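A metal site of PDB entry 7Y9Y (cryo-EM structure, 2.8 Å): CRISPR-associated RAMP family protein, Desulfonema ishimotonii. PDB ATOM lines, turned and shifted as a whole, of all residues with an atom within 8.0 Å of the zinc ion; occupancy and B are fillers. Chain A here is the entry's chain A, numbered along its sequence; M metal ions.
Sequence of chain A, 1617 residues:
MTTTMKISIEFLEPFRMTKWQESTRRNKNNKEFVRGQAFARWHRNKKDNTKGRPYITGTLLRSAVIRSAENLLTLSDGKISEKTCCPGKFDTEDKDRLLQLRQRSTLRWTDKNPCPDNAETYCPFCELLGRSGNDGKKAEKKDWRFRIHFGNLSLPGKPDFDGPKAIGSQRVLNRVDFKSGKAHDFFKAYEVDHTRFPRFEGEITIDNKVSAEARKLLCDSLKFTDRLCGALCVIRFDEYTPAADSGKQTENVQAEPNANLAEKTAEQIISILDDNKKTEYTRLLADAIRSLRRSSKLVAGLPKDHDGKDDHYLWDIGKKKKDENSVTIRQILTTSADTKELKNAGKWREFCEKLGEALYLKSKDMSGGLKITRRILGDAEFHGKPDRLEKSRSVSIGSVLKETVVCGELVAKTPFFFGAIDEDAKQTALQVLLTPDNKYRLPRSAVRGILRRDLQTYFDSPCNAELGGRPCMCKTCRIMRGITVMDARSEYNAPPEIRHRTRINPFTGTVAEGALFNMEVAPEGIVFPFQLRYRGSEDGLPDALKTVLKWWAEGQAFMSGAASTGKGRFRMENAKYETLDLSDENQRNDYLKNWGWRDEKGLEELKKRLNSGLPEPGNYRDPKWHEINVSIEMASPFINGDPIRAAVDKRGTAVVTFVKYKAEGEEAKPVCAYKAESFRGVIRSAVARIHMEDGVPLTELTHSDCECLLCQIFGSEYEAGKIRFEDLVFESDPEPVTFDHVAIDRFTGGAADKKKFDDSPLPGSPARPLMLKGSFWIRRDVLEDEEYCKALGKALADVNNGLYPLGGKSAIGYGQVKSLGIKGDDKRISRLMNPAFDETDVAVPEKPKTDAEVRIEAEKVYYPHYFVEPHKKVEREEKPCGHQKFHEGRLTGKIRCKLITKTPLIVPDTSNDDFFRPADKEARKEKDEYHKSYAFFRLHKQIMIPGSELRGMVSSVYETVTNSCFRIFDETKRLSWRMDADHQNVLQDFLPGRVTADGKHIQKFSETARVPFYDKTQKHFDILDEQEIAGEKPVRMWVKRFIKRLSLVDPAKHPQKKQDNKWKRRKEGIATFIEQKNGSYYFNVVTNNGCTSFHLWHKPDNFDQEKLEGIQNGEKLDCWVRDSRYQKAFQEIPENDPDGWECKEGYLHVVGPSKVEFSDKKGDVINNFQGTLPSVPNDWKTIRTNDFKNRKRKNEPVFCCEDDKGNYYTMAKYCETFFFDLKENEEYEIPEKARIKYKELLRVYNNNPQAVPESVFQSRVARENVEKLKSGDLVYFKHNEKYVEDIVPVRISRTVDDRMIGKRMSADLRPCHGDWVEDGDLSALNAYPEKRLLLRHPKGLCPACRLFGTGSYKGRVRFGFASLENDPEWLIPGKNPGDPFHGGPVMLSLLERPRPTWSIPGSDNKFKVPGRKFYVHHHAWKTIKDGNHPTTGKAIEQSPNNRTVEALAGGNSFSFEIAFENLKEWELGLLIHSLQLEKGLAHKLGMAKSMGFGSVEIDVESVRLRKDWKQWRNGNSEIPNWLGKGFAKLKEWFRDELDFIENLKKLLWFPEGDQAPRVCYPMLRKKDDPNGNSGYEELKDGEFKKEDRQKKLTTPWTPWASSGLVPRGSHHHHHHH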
ATOM      1  N   LYS A  83      -7.076 -11.168  -4.863  1.00  0.00           N
ATOM      2  CA  LYS A  83      -6.383 -10.010  -4.321  1.00  0.00           C
ATOM      3  C   LYS A  83      -7.326  -9.146  -3.478  1.00  0.00           C
ATOM      4  O   LYS A  83      -8.538  -9.127  -3.666  1.00  0.00           O
ATOM      5  CB  LYS A  83      -5.784  -9.168  -5.449  1.00  0.00           C
ATOM      6  CG  LYS A  83      -4.577  -9.806  -6.116  1.00  0.00           C
ATOM      7  CD  LYS A  83      -3.721  -8.758  -6.800  1.00  0.00           C
ATOM      8  CE  LYS A  83      -3.106  -7.801  -5.790  1.00  0.00           C
ATOM      9  NZ  LYS A  83      -2.221  -6.794  -6.438  1.00  0.00           N
ATOM     10  N   THR A  84      -6.729  -8.430  -2.527  1.00  0.00           N
ATOM     11  CA  THR A  84      -7.426  -7.461  -1.684  1.00  0.00           C
ATOM     12  C   THR A  84      -6.997  -6.051  -2.082  1.00  0.00           C
ATOM     13  O   THR A  84      -5.948  -5.858  -2.697  1.00  0.00           O
ATOM     14  CB  THR A  84      -7.122  -7.718  -0.200  1.00  0.00           C
ATOM     15  OG1 THR A  84      -6.984  -9.126   0.022  1.00  0.00           O
ATOM     16  CG2 THR A  84      -8.254  -7.193   0.673  1.00  0.00           C
ATOM     17  N   CYS A  85      -7.827  -5.084  -1.718  1.00  0.00           N
ATOM     18  CA  CYS A  85      -7.611  -3.697  -2.126  1.00  0.00           C
ATOM     19  C   CYS A  85      -7.466  -2.800  -0.913  1.00  0.00           C
ATOM     20  O   CYS A  85      -8.193  -2.958   0.081  1.00  0.00           O
ATOM     21  CB  CYS A  85      -8.766  -3.190  -3.004  1.00  0.00           C
ATOM     22  SG  CYS A  85      -8.947  -4.057  -4.575  1.00  0.00           S
ATOM     23  N   CYS A  86      -6.528  -1.851  -0.992  1.00  0.00           N
ATOM     24  CA  CYS A  86      -6.390  -0.829   0.022  1.00  0.00           C
ATOM     25  C   CYS A  86      -7.485   0.216  -0.152  1.00  0.00           C
ATOM     26  O   CYS A  86      -8.173   0.248  -1.181  1.00  0.00           O
ATOM     27  CB  CYS A  86      -5.017  -0.171  -0.075  1.00  0.00           C
ATOM     28  SG  CYS A  86      -4.845   0.997  -1.441  1.00  0.00           S
ATOM     29  N   PRO A  87      -7.689   1.092   0.843  1.00  0.00           N
ATOM     30  CA  PRO A  87      -8.727   2.129   0.705  1.00  0.00           C
ATOM     31  C   PRO A  87      -8.469   3.132  -0.409  1.00  0.00           C
ATOM     32  O   PRO A  87      -9.371   3.917  -0.726  1.00  0.00           O
ATOM     33  CB  PRO A  87      -8.658   2.751   2.085  1.00  0.00           C
ATOM     34  CG  PRO A  87      -7.157   2.726   2.123  1.00  0.00           C
ATOM     35  CD  PRO A  87      -7.134   1.272   2.195  1.00  0.00           C
ATOM     36  N   GLY A  88      -7.283   3.142  -1.003  1.00  0.00           N
ATOM     37  CA  GLY A  88      -6.945   4.112  -2.022  1.00  0.00           C
ATOM     38  C   GLY A  88      -6.485   5.439  -1.439  1.00  0.00           C
ATOM     39  O   GLY A  88      -6.585   5.694  -0.234  1.00  0.00           O
ATOM     40  N   LYS A  89      -5.980   6.303  -2.319  1.00  0.00           N
ATOM     41  CA  LYS A  89      -5.452   7.590  -1.914  1.00  0.00           C
ATOM     42  C   LYS A  89      -6.247   8.694  -2.593  1.00  0.00           C
ATOM     43  O   LYS A  89      -6.396   8.691  -3.820  1.00  0.00           O
ATOM     44  CB  LYS A  89      -3.967   7.724  -2.253  1.00  0.00           C
ATOM     45  CG  LYS A  89      -3.418   9.129  -2.089  1.00  0.00           C
ATOM     46  CD  LYS A  89      -1.902   9.126  -2.064  1.00  0.00           C
ATOM     47  CE  LYS A  89      -1.369   8.530  -0.772  1.00  0.00           C
ATOM     48  NZ  LYS A  89       0.101   8.783  -0.597  1.00  0.00           N
ATOM     49  N   TRP A 109     -13.775  -0.032   3.270  1.00  0.00           N
ATOM     50  CA  TRP A 109     -13.950  -1.472   3.424  1.00  0.00           C
ATOM     51  C   TRP A 109     -12.907  -2.070   4.362  1.00  0.00           C
ATOM     52  O   TRP A 109     -13.234  -2.846   5.250  1.00  0.00           O
ATOM     53  CB  TRP A 109     -13.904  -2.182   2.060  1.00  0.00           C
ATOM     54  CG  TRP A 109     -12.876  -1.651   1.106  1.00  0.00           C
ATOM     55  CD1 TRP A 109     -11.601  -2.106   0.958  1.00  0.00           C
ATOM     56  CD2 TRP A 109     -13.036  -0.613   0.138  1.00  0.00           C
ATOM     57  NE1 TRP A 109     -10.949  -1.403  -0.022  1.00  0.00           N
ATOM     58  CE2 TRP A 109     -11.819  -0.472  -0.546  1.00  0.00           C
ATOM     59  CE3 TRP A 109     -14.099   0.228  -0.209  1.00  0.00           C
ATOM     60  CZ2 TRP A 109     -11.623   0.469  -1.556  1.00  0.00           C
ATOM     61  CZ3 TRP A 109     -13.907   1.155  -1.210  1.00  0.00           C
ATOM     62  CH2 TRP A 109     -12.681   1.271  -1.873  1.00  0.00           C
ATOM     63  N   LYS A 112      -6.316  -1.116   6.487  1.00  0.00           N
ATOM     64  CA  LYS A 112      -4.878  -0.972   6.345  1.00  0.00           C
ATOM     65  C   LYS A 112      -4.558   0.274   5.537  1.00  0.00           C
ATOM     66  O   LYS A 112      -5.405   0.843   4.857  1.00  0.00           O
ATOM     67  CB  LYS A 112      -4.225  -2.201   5.682  1.00  0.00           C
ATOM     68  CG  LYS A 112      -4.298  -2.271   4.164  1.00  0.00           C
ATOM     69  CD  LYS A 112      -4.803  -3.615   3.673  1.00  0.00           C
ATOM     70  CE  LYS A 112      -6.297  -3.690   3.691  1.00  0.00           C
ATOM     71  NZ  LYS A 112      -6.816  -4.981   3.176  1.00  0.00           N
ATOM     72  N   ASN A 113      -3.303   0.714   5.638  1.00  0.00           N
ATOM     73  CA  ASN A 113      -2.867   1.933   4.981  1.00  0.00           C
ATOM     74  C   ASN A 113      -2.858   1.762   3.466  1.00  0.00           C
ATOM     75  O   ASN A 113      -2.784   0.643   2.957  1.00  0.00           O
ATOM     76  CB  ASN A 113      -1.489   2.333   5.474  1.00  0.00           C
ATOM     77  CG  ASN A 113      -1.538   3.227   6.693  1.00  0.00           C
ATOM     78  OD1 ASN A 113      -2.523   3.935   6.921  1.00  0.00           O
ATOM     79  ND2 ASN A 113      -0.475   3.207   7.489  1.00  0.00           N
ATOM     80  N   PRO A 114      -2.946   2.861   2.716  1.00  0.00           N
ATOM     81  CA  PRO A 114      -2.885   2.771   1.259  1.00  0.00           C
ATOM     82  C   PRO A 114      -1.560   2.210   0.773  1.00  0.00           C
ATOM     83  O   PRO A 114      -0.584   2.112   1.519  1.00  0.00           O
ATOM     84  CB  PRO A 114      -3.077   4.221   0.809  1.00  0.00           C
ATOM     85  CG  PRO A 114      -3.822   4.864   1.933  1.00  0.00           C
ATOM     86  CD  PRO A 114      -3.271   4.221   3.174  1.00  0.00           C
ATOM     87  N   CYS A 115      -1.541   1.846  -0.502  1.00  0.00           N
ATOM     88  CA  CYS A 115      -0.338   1.307  -1.118  1.00  0.00           C
ATOM     89  C   CYS A 115       0.785   2.347  -1.066  1.00  0.00           C
ATOM     90  O   CYS A 115       0.523   3.558  -1.135  1.00  0.00           O
ATOM     91  CB  CYS A 115      -0.603   0.896  -2.569  1.00  0.00           C
ATOM     92  SG  CYS A 115      -1.726  -0.509  -2.772  1.00  0.00           S
ATOM     93  N   PRO A 116       2.029   1.901  -0.925  1.00  0.00           N
ATOM     94  CA  PRO A 116       3.149   2.854  -0.863  1.00  0.00           C
ATOM     95  C   PRO A 116       3.223   3.701  -2.122  1.00  0.00           C
ATOM     96  O   PRO A 116       2.895   3.250  -3.220  1.00  0.00           O
ATOM     97  CB  PRO A 116       4.370   1.942  -0.724  1.00  0.00           C
ATOM     98  CG  PRO A 116       3.844   0.688  -0.105  1.00  0.00           C
ATOM     99  CD  PRO A 116       2.465   0.524  -0.673  1.00  0.00           C
ATOM    100  N   THR A 121       4.420  -3.584  -6.588  1.00  0.00           N
ATOM    101  CA  THR A 121       3.102  -4.154  -6.784  1.00  0.00           C
ATOM    102  C   THR A 121       2.043  -3.213  -6.209  1.00  0.00           C
ATOM    103  O   THR A 121       2.184  -2.713  -5.098  1.00  0.00           O
ATOM    104  CB  THR A 121       2.980  -5.522  -6.113  1.00  0.00           C
ATOM    105  OG1 THR A 121       3.089  -5.379  -4.695  1.00  0.00           O
ATOM    106  CG2 THR A 121       4.089  -6.451  -6.606  1.00  0.00           C
ATOM    107  N   TYR A 122       0.982  -2.988  -6.985  1.00  0.00           N
ATOM    108  CA  TYR A 122      -0.117  -2.147  -6.577  1.00  0.00           C
ATOM    109  C   TYR A 122      -1.408  -2.962  -6.571  1.00  0.00           C
ATOM    110  O   TYR A 122      -1.594  -3.866  -7.387  1.00  0.00           O
ATOM    111  CB  TYR A 122      -0.286  -0.940  -7.510  1.00  0.00           C
ATOM    112  CG  TYR A 122       0.499   0.284  -7.086  1.00  0.00           C
ATOM    113  CD1 TYR A 122       1.870   0.361  -7.273  1.00  0.00           C
ATOM    114  CD2 TYR A 122      -0.145   1.367  -6.510  1.00  0.00           C
ATOM    115  CE1 TYR A 122       2.578   1.473  -6.889  1.00  0.00           C
ATOM    116  CE2 TYR A 122       0.561   2.493  -6.128  1.00  0.00           C
ATOM    117  CZ  TYR A 122       1.920   2.544  -6.326  1.00  0.00           C
ATOM    118  OH  TYR A 122       2.627   3.656  -5.942  1.00  0.00           O
ATOM    119  N   CYS A 123      -2.293  -2.633  -5.637  1.00  0.00           N
ATOM    120  CA  CYS A 123      -3.580  -3.301  -5.560  1.00  0.00           C
ATOM    121  C   CYS A 123      -4.435  -2.921  -6.761  1.00  0.00           C
ATOM    122  O   CYS A 123      -4.225  -1.872  -7.377  1.00  0.00           O
ATOM    123  CB  CYS A 123      -4.283  -2.939  -4.248  1.00  0.00           C
ATOM    124  SG  CYS A 123      -5.269  -1.436  -4.308  1.00  0.00           S
ATOM    125  N   PRO A 124      -5.402  -3.765  -7.137  1.00  0.00           N
ATOM    126  CA  PRO A 124      -6.204  -3.484  -8.335  1.00  0.00           C
ATOM    127  C   PRO A 124      -6.938  -2.155  -8.277  1.00  0.00           C
ATOM    128  O   PRO A 124      -7.126  -1.522  -9.329  1.00  0.00           O
ATOM    129  CB  PRO A 124      -7.187  -4.658  -8.376  1.00  0.00           C
ATOM    130  CG  PRO A 124      -6.462  -5.766  -7.691  1.00  0.00           C
ATOM    131  CD  PRO A 124      -5.716  -5.099  -6.575  1.00  0.00           C
ATOM    132  N   PHE A 125      -7.364  -1.705  -7.097  1.00  0.00           N
ATOM    133  CA  PHE A 125      -8.051  -0.429  -7.000  1.00  0.00           C
ATOM    134  C   PHE A 125      -7.126   0.721  -7.362  1.00  0.00           C
ATOM    135  O   PHE A 125      -7.552   1.720  -7.940  1.00  0.00           O
ATOM    136  CB  PHE A 125      -8.635  -0.252  -5.591  1.00  0.00           C
ATOM    137  CG  PHE A 125      -9.425   1.004  -5.411  1.00  0.00           C
ATOM    138  CD1 PHE A 125     -10.701   1.113  -5.952  1.00  0.00           C
ATOM    139  CD2 PHE A 125      -8.928   2.052  -4.670  1.00  0.00           C
ATOM    140  CE1 PHE A 125     -11.442   2.266  -5.785  1.00  0.00           C
ATOM    141  CE2 PHE A 125      -9.676   3.205  -4.495  1.00  0.00           C
ATOM    142  CZ  PHE A 125     -10.926   3.310  -5.054  1.00  0.00           C
ATOM    143  N   CYS A 126      -5.835   0.588  -7.031  1.00  0.00           N
ATOM    144  CA  CYS A 126      -4.870   1.620  -7.414  1.00  0.00           C
ATOM    145  C   CYS A 126      -4.582   1.586  -8.900  1.00  0.00           C
ATOM    146  O   CYS A 126      -4.389   2.638  -9.530  1.00  0.00           O
ATOM    147  CB  CYS A 126      -3.587   1.451  -6.605  1.00  0.00           C
ATOM    148  SG  CYS A 126      -3.724   1.952  -4.878  1.00  0.00           S
ATOM    149  N   GLU A 127      -4.540   0.392  -9.502  1.00  0.00           N
ATOM    150  CA  GLU A 127      -4.375   0.305 -10.950  1.00  0.00           C
ATOM    151  C   GLU A 127      -5.548   0.944 -11.670  1.00  0.00           C
ATOM    152  O   GLU A 127      -5.366   1.630 -12.682  1.00  0.00           O
ATOM    153  CB  GLU A 127      -4.211  -1.151 -11.388  1.00  0.00           C
ATOM    154  CG  GLU A 127      -3.181  -1.943 -10.596  1.00  0.00           C
ATOM    155  CD  GLU A 127      -2.904  -3.294 -11.212  1.00  0.00           C
ATOM    156  OE1 GLU A 127      -2.588  -3.346 -12.413  1.00  0.00           O
ATOM    157  OE2 GLU A 127      -3.004  -4.312 -10.490  1.00  0.00           O
ATOM    158  N   LEU A 129      -7.351   3.321 -10.336  1.00  0.00           N
ATOM    159  CA  LEU A 129      -7.152   4.737 -10.076  1.00  0.00           C
ATOM    160  C   LEU A 129      -6.119   5.334 -11.024  1.00  0.00           C
ATOM    161  O   LEU A 129      -6.286   6.461 -11.500  1.00  0.00           O
ATOM    162  CB  LEU A 129      -6.716   4.945  -8.628  1.00  0.00           C
ATOM    163  CG  LEU A 129      -7.784   5.009  -7.539  1.00  0.00           C
ATOM    164  CD1 LEU A 129      -7.124   5.022  -6.168  1.00  0.00           C
ATOM    165  CD2 LEU A 129      -8.647   6.238  -7.710  1.00  0.00           C
ATOM    166  N   ARG A 131      -2.571   4.939 -10.085  1.00  0.00           N
ATOM    167  CA  ARG A 131      -1.359   5.188  -9.303  1.00  0.00           C
ATOM    168  C   ARG A 131      -0.156   4.471  -9.896  1.00  0.00           C
ATOM    169  O   ARG A 131       0.947   5.034  -9.935  1.00  0.00           O
ATOM    170  CB  ARG A 131      -1.575   4.760  -7.855  1.00  0.00           C
ATOM    171  CG  ARG A 131      -2.941   5.120  -7.302  1.00  0.00           C
ATOM    172  CD  ARG A 131      -2.855   6.225  -6.253  1.00  0.00           C
ATOM    173  NE  ARG A 131      -1.633   6.144  -5.468  1.00  0.00           N
ATOM    174  CZ  ARG A 131      -1.455   5.341  -4.428  1.00  0.00           C
ATOM    175  NH1 ARG A 131      -2.415   4.531  -4.011  1.00  0.00           N
ATOM    176  NH2 ARG A 131      -0.293   5.362  -3.784  1.00  0.00           N
HETATM  177 ZN    ZN M   1      -3.865   0.185  -3.379  1.00  0.00          ZN
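Within 4 Å of the zinc ion: Cys 86, Cys 115, Cys 123 and Cys 126.
N of Gly 88 lies close to SG of Cys 86 (3.3 Å).
The backbone carbonyl oxygen (O) of Cys 86 lies within hydrogen-bond range of the indole nitrogen (NE1) of Trp 109 (3.4 Å).
The backbone NH (N) of Arg 131 is in hydrogen-bond range of the backbone carbonyl oxygen (O) of Cys 126 (3.0 Å).
The backbone carbonyl oxygen (O) of Cys 115 lies within hydrogen-bond range of the guanidinium group (NH2) of Arg 131 (3.3 Å).
The side-chain sulfur (SG) of Cys 123 sits close to the backbone NH (N) of Phe 125, at 3.5 Å.
The zinc ion is bound by the side-chain sulfur (SG) of Cys 86 (2.3 Å), the side-chain sulfur (SG) of Cys 126 (2.3 Å), the side-chain sulfur (SG) of Cys 115 (2.3 Å) and the side-chain sulfur (SG) of Cys 123 (2.3 Å).
The zinc ion has four donor atoms within binding distance.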
